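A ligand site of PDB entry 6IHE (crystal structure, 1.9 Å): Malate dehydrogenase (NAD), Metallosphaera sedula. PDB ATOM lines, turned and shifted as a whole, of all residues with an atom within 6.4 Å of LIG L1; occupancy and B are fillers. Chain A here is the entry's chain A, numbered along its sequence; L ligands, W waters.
Residues that only touch LIG L1: Ile 211, Pro 207 and His 171. Eight residues have an atom within 4 Å of LIG L1: Arg 81, Arg 87, Asn 119, Arg 147, His 171, Pro 207, Ile 211 and Thr 217. The nearest printed residue that does not touch LIG L1 is Pro 221 (4.02 Å).
Water W2 lies within hydrogen-bond range of an oxygen (O4) of LIG L1 (2.5 Å), an oxygen (O13) of LG2 L2 (2.6 Å) and the backbone NH (N) of Arg 81 (3.1 Å). Water W1 lies within hydrogen-bond range of O1 of LIG L1 (2.8 Å), N7 of LG2 L2 (2.8 Å) and OE1 of Glu 144 (3.5 Å).
OD1 of Asn 119 is in hydrogen-bond range of NE2 of His 171 (3.4 Å). The backbone NH (N) of Val 121 lies within hydrogen-bond range of the side-chain amide oxygen (OD1) of Asn 119, 3.0 Å away. NE2 of His 171 is in hydrogen-bond range of NE of Arg 87, at 3.3 Å.
An oxygen (O13) of LG2 L2 lies within hydrogen-bond range of the side-chain amide nitrogen of Asn 119, 3.0 Å away. The guanidinium group of Arg 147 lies within salt-bridge range of an oxygen (O1) of LIG L1 (2.6 Å). OG1 of Thr 217 lies within hydrogen-bond range of O2 of LIG L1, at 2.7 Å. O1 of LIG L1 is in salt-bridge range of NH2 of Arg 87 (3.0 Å). ND2 of Asn 119 sits at hydrogen-bond distance from O3 of LIG L1. The guanidinium group of Arg 81 lies within salt-bridge range of an oxygen (O5) of LIG L1 (2.8 Å). The backbone NH of Asn 119 lies within hydrogen-bond range of an oxygen (O12) of LG2 L2 (3.0 Å).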
ATOM      1  N   PRO A  80     -24.122  21.283 -10.650  1.00  0.00           N
ATOM      2  CA  PRO A  80     -24.487  22.643 -10.279  1.00  0.00           C
ATOM      3  C   PRO A  80     -25.808  22.585  -9.546  1.00  0.00           C
ATOM      4  O   PRO A  80     -26.402  21.558  -9.481  1.00  0.00           O
ATOM      5  CB  PRO A  80     -24.717  23.315 -11.605  1.00  0.00           C
ATOM      6  CG  PRO A  80     -25.182  22.234 -12.467  1.00  0.00           C
ATOM      7  CD  PRO A  80     -24.368  21.055 -12.069  1.00  0.00           C
ATOM      8  N   ARG A  81     -26.232  23.715  -9.026  1.00  0.00           N
ATOM      9  CA  ARG A  81     -27.477  23.848  -8.300  1.00  0.00           C
ATOM     10  C   ARG A  81     -28.715  23.886  -9.174  1.00  0.00           C
ATOM     11  O   ARG A  81     -28.689  24.326 -10.284  1.00  0.00           O
ATOM     12  CB  ARG A  81     -27.461  25.151  -7.536  1.00  0.00           C
ATOM     13  CG  ARG A  81     -26.765  25.115  -6.217  1.00  0.00           C
ATOM     14  CD  ARG A  81     -27.425  26.056  -5.249  1.00  0.00           C
ATOM     15  NE  ARG A  81     -27.133  27.447  -5.558  1.00  0.00           N
ATOM     16  CZ  ARG A  81     -27.665  28.470  -4.920  1.00  0.00           C
ATOM     17  NH1 ARG A  81     -28.525  28.277  -3.964  1.00  0.00           N
ATOM     18  NH2 ARG A  81     -27.337  29.699  -5.245  1.00  0.00           N
ATOM     19  N   ARG A  87     -26.032  25.405  -1.799  1.00  0.00           N
ATOM     20  CA  ARG A  87     -24.792  25.001  -2.432  1.00  0.00           C
ATOM     21  C   ARG A  87     -24.198  23.811  -1.723  1.00  0.00           C
ATOM     22  O   ARG A  87     -23.637  22.933  -2.328  1.00  0.00           O
ATOM     23  CB  ARG A  87     -23.764  26.126  -2.486  1.00  0.00           C
ATOM     24  CG  ARG A  87     -24.123  27.316  -3.338  1.00  0.00           C
ATOM     25  CD  ARG A  87     -23.060  28.383  -3.195  1.00  0.00           C
ATOM     26  NE  ARG A  87     -23.288  29.565  -3.986  1.00  0.00           N
ATOM     27  CZ  ARG A  87     -24.155  30.519  -3.697  1.00  0.00           C
ATOM     28  NH1 ARG A  87     -24.902  30.441  -2.618  1.00  0.00           N
ATOM     29  NH2 ARG A  87     -24.271  31.568  -4.469  1.00  0.00           N
ATOM     30  N   LEU A  90     -24.674  19.873  -2.527  1.00  0.00           N
ATOM     31  CA  LEU A  90     -23.837  19.207  -3.507  1.00  0.00           C
ATOM     32  C   LEU A  90     -22.602  18.510  -2.894  1.00  0.00           C
ATOM     33  O   LEU A  90     -21.852  17.877  -3.636  1.00  0.00           O
ATOM     34  CB  LEU A  90     -23.365  20.251  -4.545  1.00  0.00           C
ATOM     35  CG  LEU A  90     -24.467  20.944  -5.310  1.00  0.00           C
ATOM     36  CD1 LEU A  90     -24.009  22.277  -5.873  1.00  0.00           C
ATOM     37  CD2 LEU A  90     -25.035  20.019  -6.401  1.00  0.00           C
ATOM     38  N   VAL A 117     -13.594  26.071  -8.289  1.00  0.00           N
ATOM     39  CA  VAL A 117     -14.749  26.777  -8.735  1.00  0.00           C
ATOM     40  C   VAL A 117     -16.018  25.987  -8.418  1.00  0.00           C
ATOM     41  O   VAL A 117     -17.060  26.599  -8.111  1.00  0.00           O
ATOM     42  CB  VAL A 117     -14.682  27.029 -10.233  1.00  0.00           C
ATOM     43  CG1 VAL A 117     -15.997  27.580 -10.745  1.00  0.00           C
ATOM     44  CG2 VAL A 117     -13.499  27.874 -10.554  1.00  0.00           C
ATOM     45  N   ASN A 119     -18.947  23.898  -6.685  1.00  0.00           N
ATOM     46  CA  ASN A 119     -19.578  24.037  -5.360  1.00  0.00           C
ATOM     47  C   ASN A 119     -19.765  22.716  -4.571  1.00  0.00           C
ATOM     48  O   ASN A 119     -19.810  21.675  -5.150  1.00  0.00           O
ATOM     49  CB  ASN A 119     -20.937  24.740  -5.511  1.00  0.00           C
ATOM     50  CG  ASN A 119     -20.824  26.243  -5.587  1.00  0.00           C
ATOM     51  OD1 ASN A 119     -20.213  26.840  -4.751  1.00  0.00           O
ATOM     52  ND2 ASN A 119     -21.417  26.843  -6.579  1.00  0.00           N
ATOM     53  N   VAL A 121     -18.056  25.531  -3.151  1.00  0.00           N
ATOM     54  CA  VAL A 121     -16.697  25.956  -3.355  1.00  0.00           C
ATOM     55  C   VAL A 121     -15.621  25.914  -2.292  1.00  0.00           C
ATOM     56  O   VAL A 121     -14.576  25.423  -2.563  1.00  0.00           O
ATOM     57  CB  VAL A 121     -16.596  27.226  -4.206  1.00  0.00           C
ATOM     58  CG1 VAL A 121     -16.812  28.444  -3.359  1.00  0.00           C
ATOM     59  CG2 VAL A 121     -15.273  27.266  -4.911  1.00  0.00           C
ATOM     60  N   VAL A 143     -16.840  36.693  -5.946  1.00  0.00           N
ATOM     61  CA  VAL A 143     -18.033  36.892  -6.788  1.00  0.00           C
ATOM     62  C   VAL A 143     -19.055  37.773  -6.019  1.00  0.00           C
ATOM     63  O   VAL A 143     -19.562  38.758  -6.546  1.00  0.00           O
ATOM     64  CB  VAL A 143     -18.682  35.572  -7.212  1.00  0.00           C
ATOM     65  CG1 VAL A 143     -19.967  35.813  -8.086  1.00  0.00           C
ATOM     66  CG2 VAL A 143     -17.674  34.727  -8.019  1.00  0.00           C
ATOM     67  N   GLU A 144     -19.244  37.433  -4.747  1.00  0.00           N
ATOM     68  CA  GLU A 144     -20.137  38.136  -3.795  1.00  0.00           C
ATOM     69  C   GLU A 144     -19.685  39.567  -3.679  1.00  0.00           C
ATOM     70  O   GLU A 144     -20.533  40.500  -3.803  1.00  0.00           O
ATOM     71  CB  GLU A 144     -20.132  37.464  -2.390  1.00  0.00           C
ATOM     72  CG  GLU A 144     -20.969  36.220  -2.268  1.00  0.00           C
ATOM     73  CD  GLU A 144     -20.507  34.997  -3.062  1.00  0.00           C
ATOM     74  OE1 GLU A 144     -19.391  35.006  -3.722  1.00  0.00           O
ATOM     75  OE2 GLU A 144     -21.308  34.003  -2.997  1.00  0.00           O
ATOM     76  N   ARG A 147     -20.719  41.477  -6.725  1.00  0.00           N
ATOM     77  CA  ARG A 147     -22.132  41.660  -6.707  1.00  0.00           C
ATOM     78  C   ARG A 147     -22.580  42.835  -5.773  1.00  0.00           C
ATOM     79  O   ARG A 147     -23.421  43.656  -6.139  1.00  0.00           O
ATOM     80  CB  ARG A 147     -22.805  40.382  -6.323  1.00  0.00           C
ATOM     81  CG  ARG A 147     -22.735  39.353  -7.424  1.00  0.00           C
ATOM     82  CD  ARG A 147     -23.193  37.982  -6.984  1.00  0.00           C
ATOM     83  NE  ARG A 147     -23.334  37.102  -8.155  1.00  0.00           N
ATOM     84  CZ  ARG A 147     -23.305  35.790  -8.095  1.00  0.00           C
ATOM     85  NH1 ARG A 147     -23.139  35.138  -6.943  1.00  0.00           N
ATOM     86  NH2 ARG A 147     -23.395  35.114  -9.241  1.00  0.00           N
ATOM     87  N   HIS A 171     -18.846  30.850   2.407  1.00  0.00           N
ATOM     88  CA  HIS A 171     -19.288  31.106   1.051  1.00  0.00           C
ATOM     89  C   HIS A 171     -20.772  31.388   0.895  1.00  0.00           C
ATOM     90  O   HIS A 171     -21.566  31.040   1.705  1.00  0.00           O
ATOM     91  CB  HIS A 171     -18.838  29.948   0.134  1.00  0.00           C
ATOM     92  CG  HIS A 171     -19.249  30.080  -1.302  1.00  0.00           C
ATOM     93  ND1 HIS A 171     -18.736  31.029  -2.137  1.00  0.00           N
ATOM     94  CD2 HIS A 171     -20.133  29.387  -2.039  1.00  0.00           C
ATOM     95  CE1 HIS A 171     -19.276  30.922  -3.320  1.00  0.00           C
ATOM     96  NE2 HIS A 171     -20.133  29.924  -3.288  1.00  0.00           N
ATOM     97  N   GLY A 172     -21.117  32.019  -0.211  1.00  0.00           N
ATOM     98  CA  GLY A 172     -22.492  32.291  -0.498  1.00  0.00           C
ATOM     99  C   GLY A 172     -23.454  32.694   0.592  1.00  0.00           C
ATOM    100  O   GLY A 172     -23.273  33.660   1.226  1.00  0.00           O
ATOM    101  N   PRO A 207     -27.826  35.109  -7.166  1.00  0.00           N
ATOM    102  CA  PRO A 207     -27.499  33.883  -7.964  1.00  0.00           C
ATOM    103  C   PRO A 207     -28.632  32.869  -8.086  1.00  0.00           C
ATOM    104  O   PRO A 207     -28.890  32.362  -9.220  1.00  0.00           O
ATOM    105  CB  PRO A 207     -26.293  33.284  -7.260  1.00  0.00           C
ATOM    106  CG  PRO A 207     -26.196  33.951  -5.941  1.00  0.00           C
ATOM    107  CD  PRO A 207     -26.846  35.310  -6.060  1.00  0.00           C
ATOM    108  N   GLY A 208     -29.357  32.644  -6.973  1.00  0.00           N
ATOM    109  CA  GLY A 208     -30.522  31.778  -6.968  1.00  0.00           C
ATOM    110  C   GLY A 208     -31.548  32.198  -7.995  1.00  0.00           C
ATOM    111  O   GLY A 208     -32.147  31.359  -8.699  1.00  0.00           O
ATOM    112  N   ILE A 211     -30.247  31.482 -11.471  1.00  0.00           N
ATOM    113  CA  ILE A 211     -30.441  30.081 -11.706  1.00  0.00           C
ATOM    114  C   ILE A 211     -31.891  29.757 -12.085  1.00  0.00           C
ATOM    115  O   ILE A 211     -32.109  29.061 -13.079  1.00  0.00           O
ATOM    116  CB  ILE A 211     -30.004  29.229 -10.501  1.00  0.00           C
ATOM    117  CG1 ILE A 211     -28.471  29.247 -10.400  1.00  0.00           C
ATOM    118  CG2 ILE A 211     -30.542  27.818 -10.708  1.00  0.00           C
ATOM    119  CD1 ILE A 211     -27.892  28.949  -9.035  1.00  0.00           C
ATOM    120  N   THR A 217     -25.536  30.533 -13.310  1.00  0.00           N
ATOM    121  CA  THR A 217     -24.767  31.749 -13.433  1.00  0.00           C
ATOM    122  C   THR A 217     -23.571  31.532 -14.385  1.00  0.00           C
ATOM    123  O   THR A 217     -22.940  30.458 -14.388  1.00  0.00           O
ATOM    124  CB  THR A 217     -24.279  32.207 -12.078  1.00  0.00           C
ATOM    125  OG1 THR A 217     -23.598  31.133 -11.448  1.00  0.00           O
ATOM    126  CG2 THR A 217     -25.495  32.639 -11.181  1.00  0.00           C
ATOM    127  N   THR A 218     -23.298  32.527 -15.222  1.00  0.00           N
ATOM    128  CA  THR A 218     -22.270  32.447 -16.210  1.00  0.00           C
ATOM    129  C   THR A 218     -21.387  33.663 -16.284  1.00  0.00           C
ATOM    130  O   THR A 218     -20.270  33.701 -15.735  1.00  0.00           O
ATOM    131  CB  THR A 218     -22.869  32.110 -17.579  1.00  0.00           C
ATOM    132  OG1 THR A 218     -23.806  33.121 -17.997  1.00  0.00           O
ATOM    133  CG2 THR A 218     -23.579  30.819 -17.505  1.00  0.00           C
ATOM    134  N   PRO A 221     -19.790  35.425 -12.697  1.00  0.00           N
ATOM    135  CA  PRO A 221     -18.688  34.690 -12.033  1.00  0.00           C
ATOM    136  C   PRO A 221     -17.569  34.257 -13.011  1.00  0.00           C
ATOM    137  O   PRO A 221     -16.405  34.234 -12.656  1.00  0.00           O
ATOM    138  CB  PRO A 221     -19.383  33.514 -11.391  1.00  0.00           C
ATOM    139  CG  PRO A 221     -20.721  33.426 -12.028  1.00  0.00           C
ATOM    140  CD  PRO A 221     -21.067  34.735 -12.610  1.00  0.00           C
HETATM  141  C1  LIG L   1     -22.794  31.803  -7.805  1.00  0.00           C
HETATM  142  O1  LIG L   1     -22.667  32.557  -6.824  1.00  0.00           O
HETATM  143  O2  LIG L   1     -23.038  32.184  -8.983  1.00  0.00           O
HETATM  144  C2  LIG L   1     -22.778  30.367  -7.324  1.00  0.00           C
HETATM  145  O3  LIG L   1     -21.684  29.907  -6.565  1.00  0.00           O
HETATM  146  C3  LIG L   1     -23.293  29.319  -8.302  1.00  0.00           C
HETATM  147  C4  LIG L   1     -24.547  28.889  -7.531  1.00  0.00           C
HETATM  148  O4  LIG L   1     -24.839  27.685  -7.274  1.00  0.00           O
HETATM  149  O5  LIG L   1     -25.247  29.837  -7.102  1.00  0.00           O
HETATM  150  P1  LG2 L   2     -22.654  22.288 -16.007  1.00  0.00           P
HETATM  151  O1  LG2 L   2     -23.551  21.070 -15.760  1.00  0.00           O
HETATM  152  O2  LG2 L   2     -22.876  23.267 -17.162  1.00  0.00           O
HETATM  153  O3  LG2 L   2     -21.192  21.686 -16.177  1.00  0.00           O
HETATM  154  C1  LG2 L   2     -20.545  20.799 -15.261  1.00  0.00           C
HETATM  155  C2  LG2 L   2     -19.466  20.167 -16.111  1.00  0.00           C
HETATM  156  O4  LG2 L   2     -18.693  19.368 -15.257  1.00  0.00           O
HETATM  157  C3  LG2 L   2     -20.099  19.284 -17.187  1.00  0.00           C
HETATM  158  O5  LG2 L   2     -19.683  19.624 -18.539  1.00  0.00           O
HETATM  159  C4  LG2 L   2     -19.738  17.899 -16.728  1.00  0.00           C
HETATM  160  O6  LG2 L   2     -19.361  16.983 -17.722  1.00  0.00           O
HETATM  161  C5  LG2 L   2     -18.488  18.168 -15.971  1.00  0.00           C
HETATM  162  N1  LG2 L   2     -18.180  17.052 -15.074  1.00  0.00           N
HETATM  163  C6  LG2 L   2     -18.965  16.445 -14.149  1.00  0.00           C
HETATM  164  N2  LG2 L   2     -18.210  15.479 -13.536  1.00  0.00           N
HETATM  165  C7  LG2 L   2     -16.956  15.490 -14.050  1.00  0.00           C
HETATM  166  C8  LG2 L   2     -15.688  14.733 -13.851  1.00  0.00           C
HETATM  167  N3  LG2 L   2     -15.681  13.765 -12.918  1.00  0.00           N
HETATM  168  N4  LG2 L   2     -14.588  15.037 -14.632  1.00  0.00           N
HETATM  169  C9  LG2 L   2     -14.670  16.038 -15.585  1.00  0.00           C
HETATM  170  N5  LG2 L   2     -15.781  16.779 -15.871  1.00  0.00           N
HETATM  171  C10 LG2 L   2     -16.926  16.527 -15.105  1.00  0.00           C
HETATM  172  O7  LG2 L   2     -22.392  23.098 -14.629  1.00  0.00           O
HETATM  173  P2  LG2 L   2     -21.737  24.604 -14.501  1.00  0.00           P
HETATM  174  O8  LG2 L   2     -22.872  25.596 -14.610  1.00  0.00           O
HETATM  175  O9  LG2 L   2     -20.586  24.784 -15.444  1.00  0.00           O
HETATM  176  O10 LG2 L   2     -21.250  24.432 -12.965  1.00  0.00           O
HETATM  177  C11 LG2 L   2     -20.161  23.629 -12.610  1.00  0.00           C
HETATM  178  C12 LG2 L   2     -19.882  23.800 -11.136  1.00  0.00           C
HETATM  179  O11 LG2 L   2     -19.459  25.151 -10.859  1.00  0.00           O
HETATM  180  C13 LG2 L   2     -21.091  23.566 -10.246  1.00  0.00           C
HETATM  181  O12 LG2 L   2     -20.686  22.985  -8.983  1.00  0.00           O
HETATM  182  C14 LG2 L   2     -21.667  24.983  -9.971  1.00  0.00           C
HETATM  183  O13 LG2 L   2     -22.463  25.044  -8.750  1.00  0.00           O
HETATM  184  C15 LG2 L   2     -20.345  25.758  -9.878  1.00  0.00           C
HETATM  185  N6  LG2 L   2     -20.338  27.228 -10.118  1.00  0.00           N
HETATM  186  C16 LG2 L   2     -19.633  27.985  -9.227  1.00  0.00           C
HETATM  187  C17 LG2 L   2     -19.490  29.366  -9.345  1.00  0.00           C
HETATM  188  C18 LG2 L   2     -18.677  30.085  -8.321  1.00  0.00           C
HETATM  189  O14 LG2 L   2     -17.810  29.538  -7.626  1.00  0.00           O
HETATM  190  N7  LG2 L   2     -18.853  31.371  -8.221  1.00  0.00           N
HETATM  191  C19 LG2 L   2     -20.154  29.985 -10.401  1.00  0.00           C
HETATM  192  C20 LG2 L   2     -20.893  29.192 -11.314  1.00  0.00           C
HETATM  193  C21 LG2 L   2     -20.983  27.813 -11.150  1.00  0.00           C
HETATM  194  O   HOH W   1     -20.032  32.362  -5.866  1.00  0.00           O
HETATM  195  O   HOH W   2     -24.633  26.291  -9.387  1.00  0.00           O
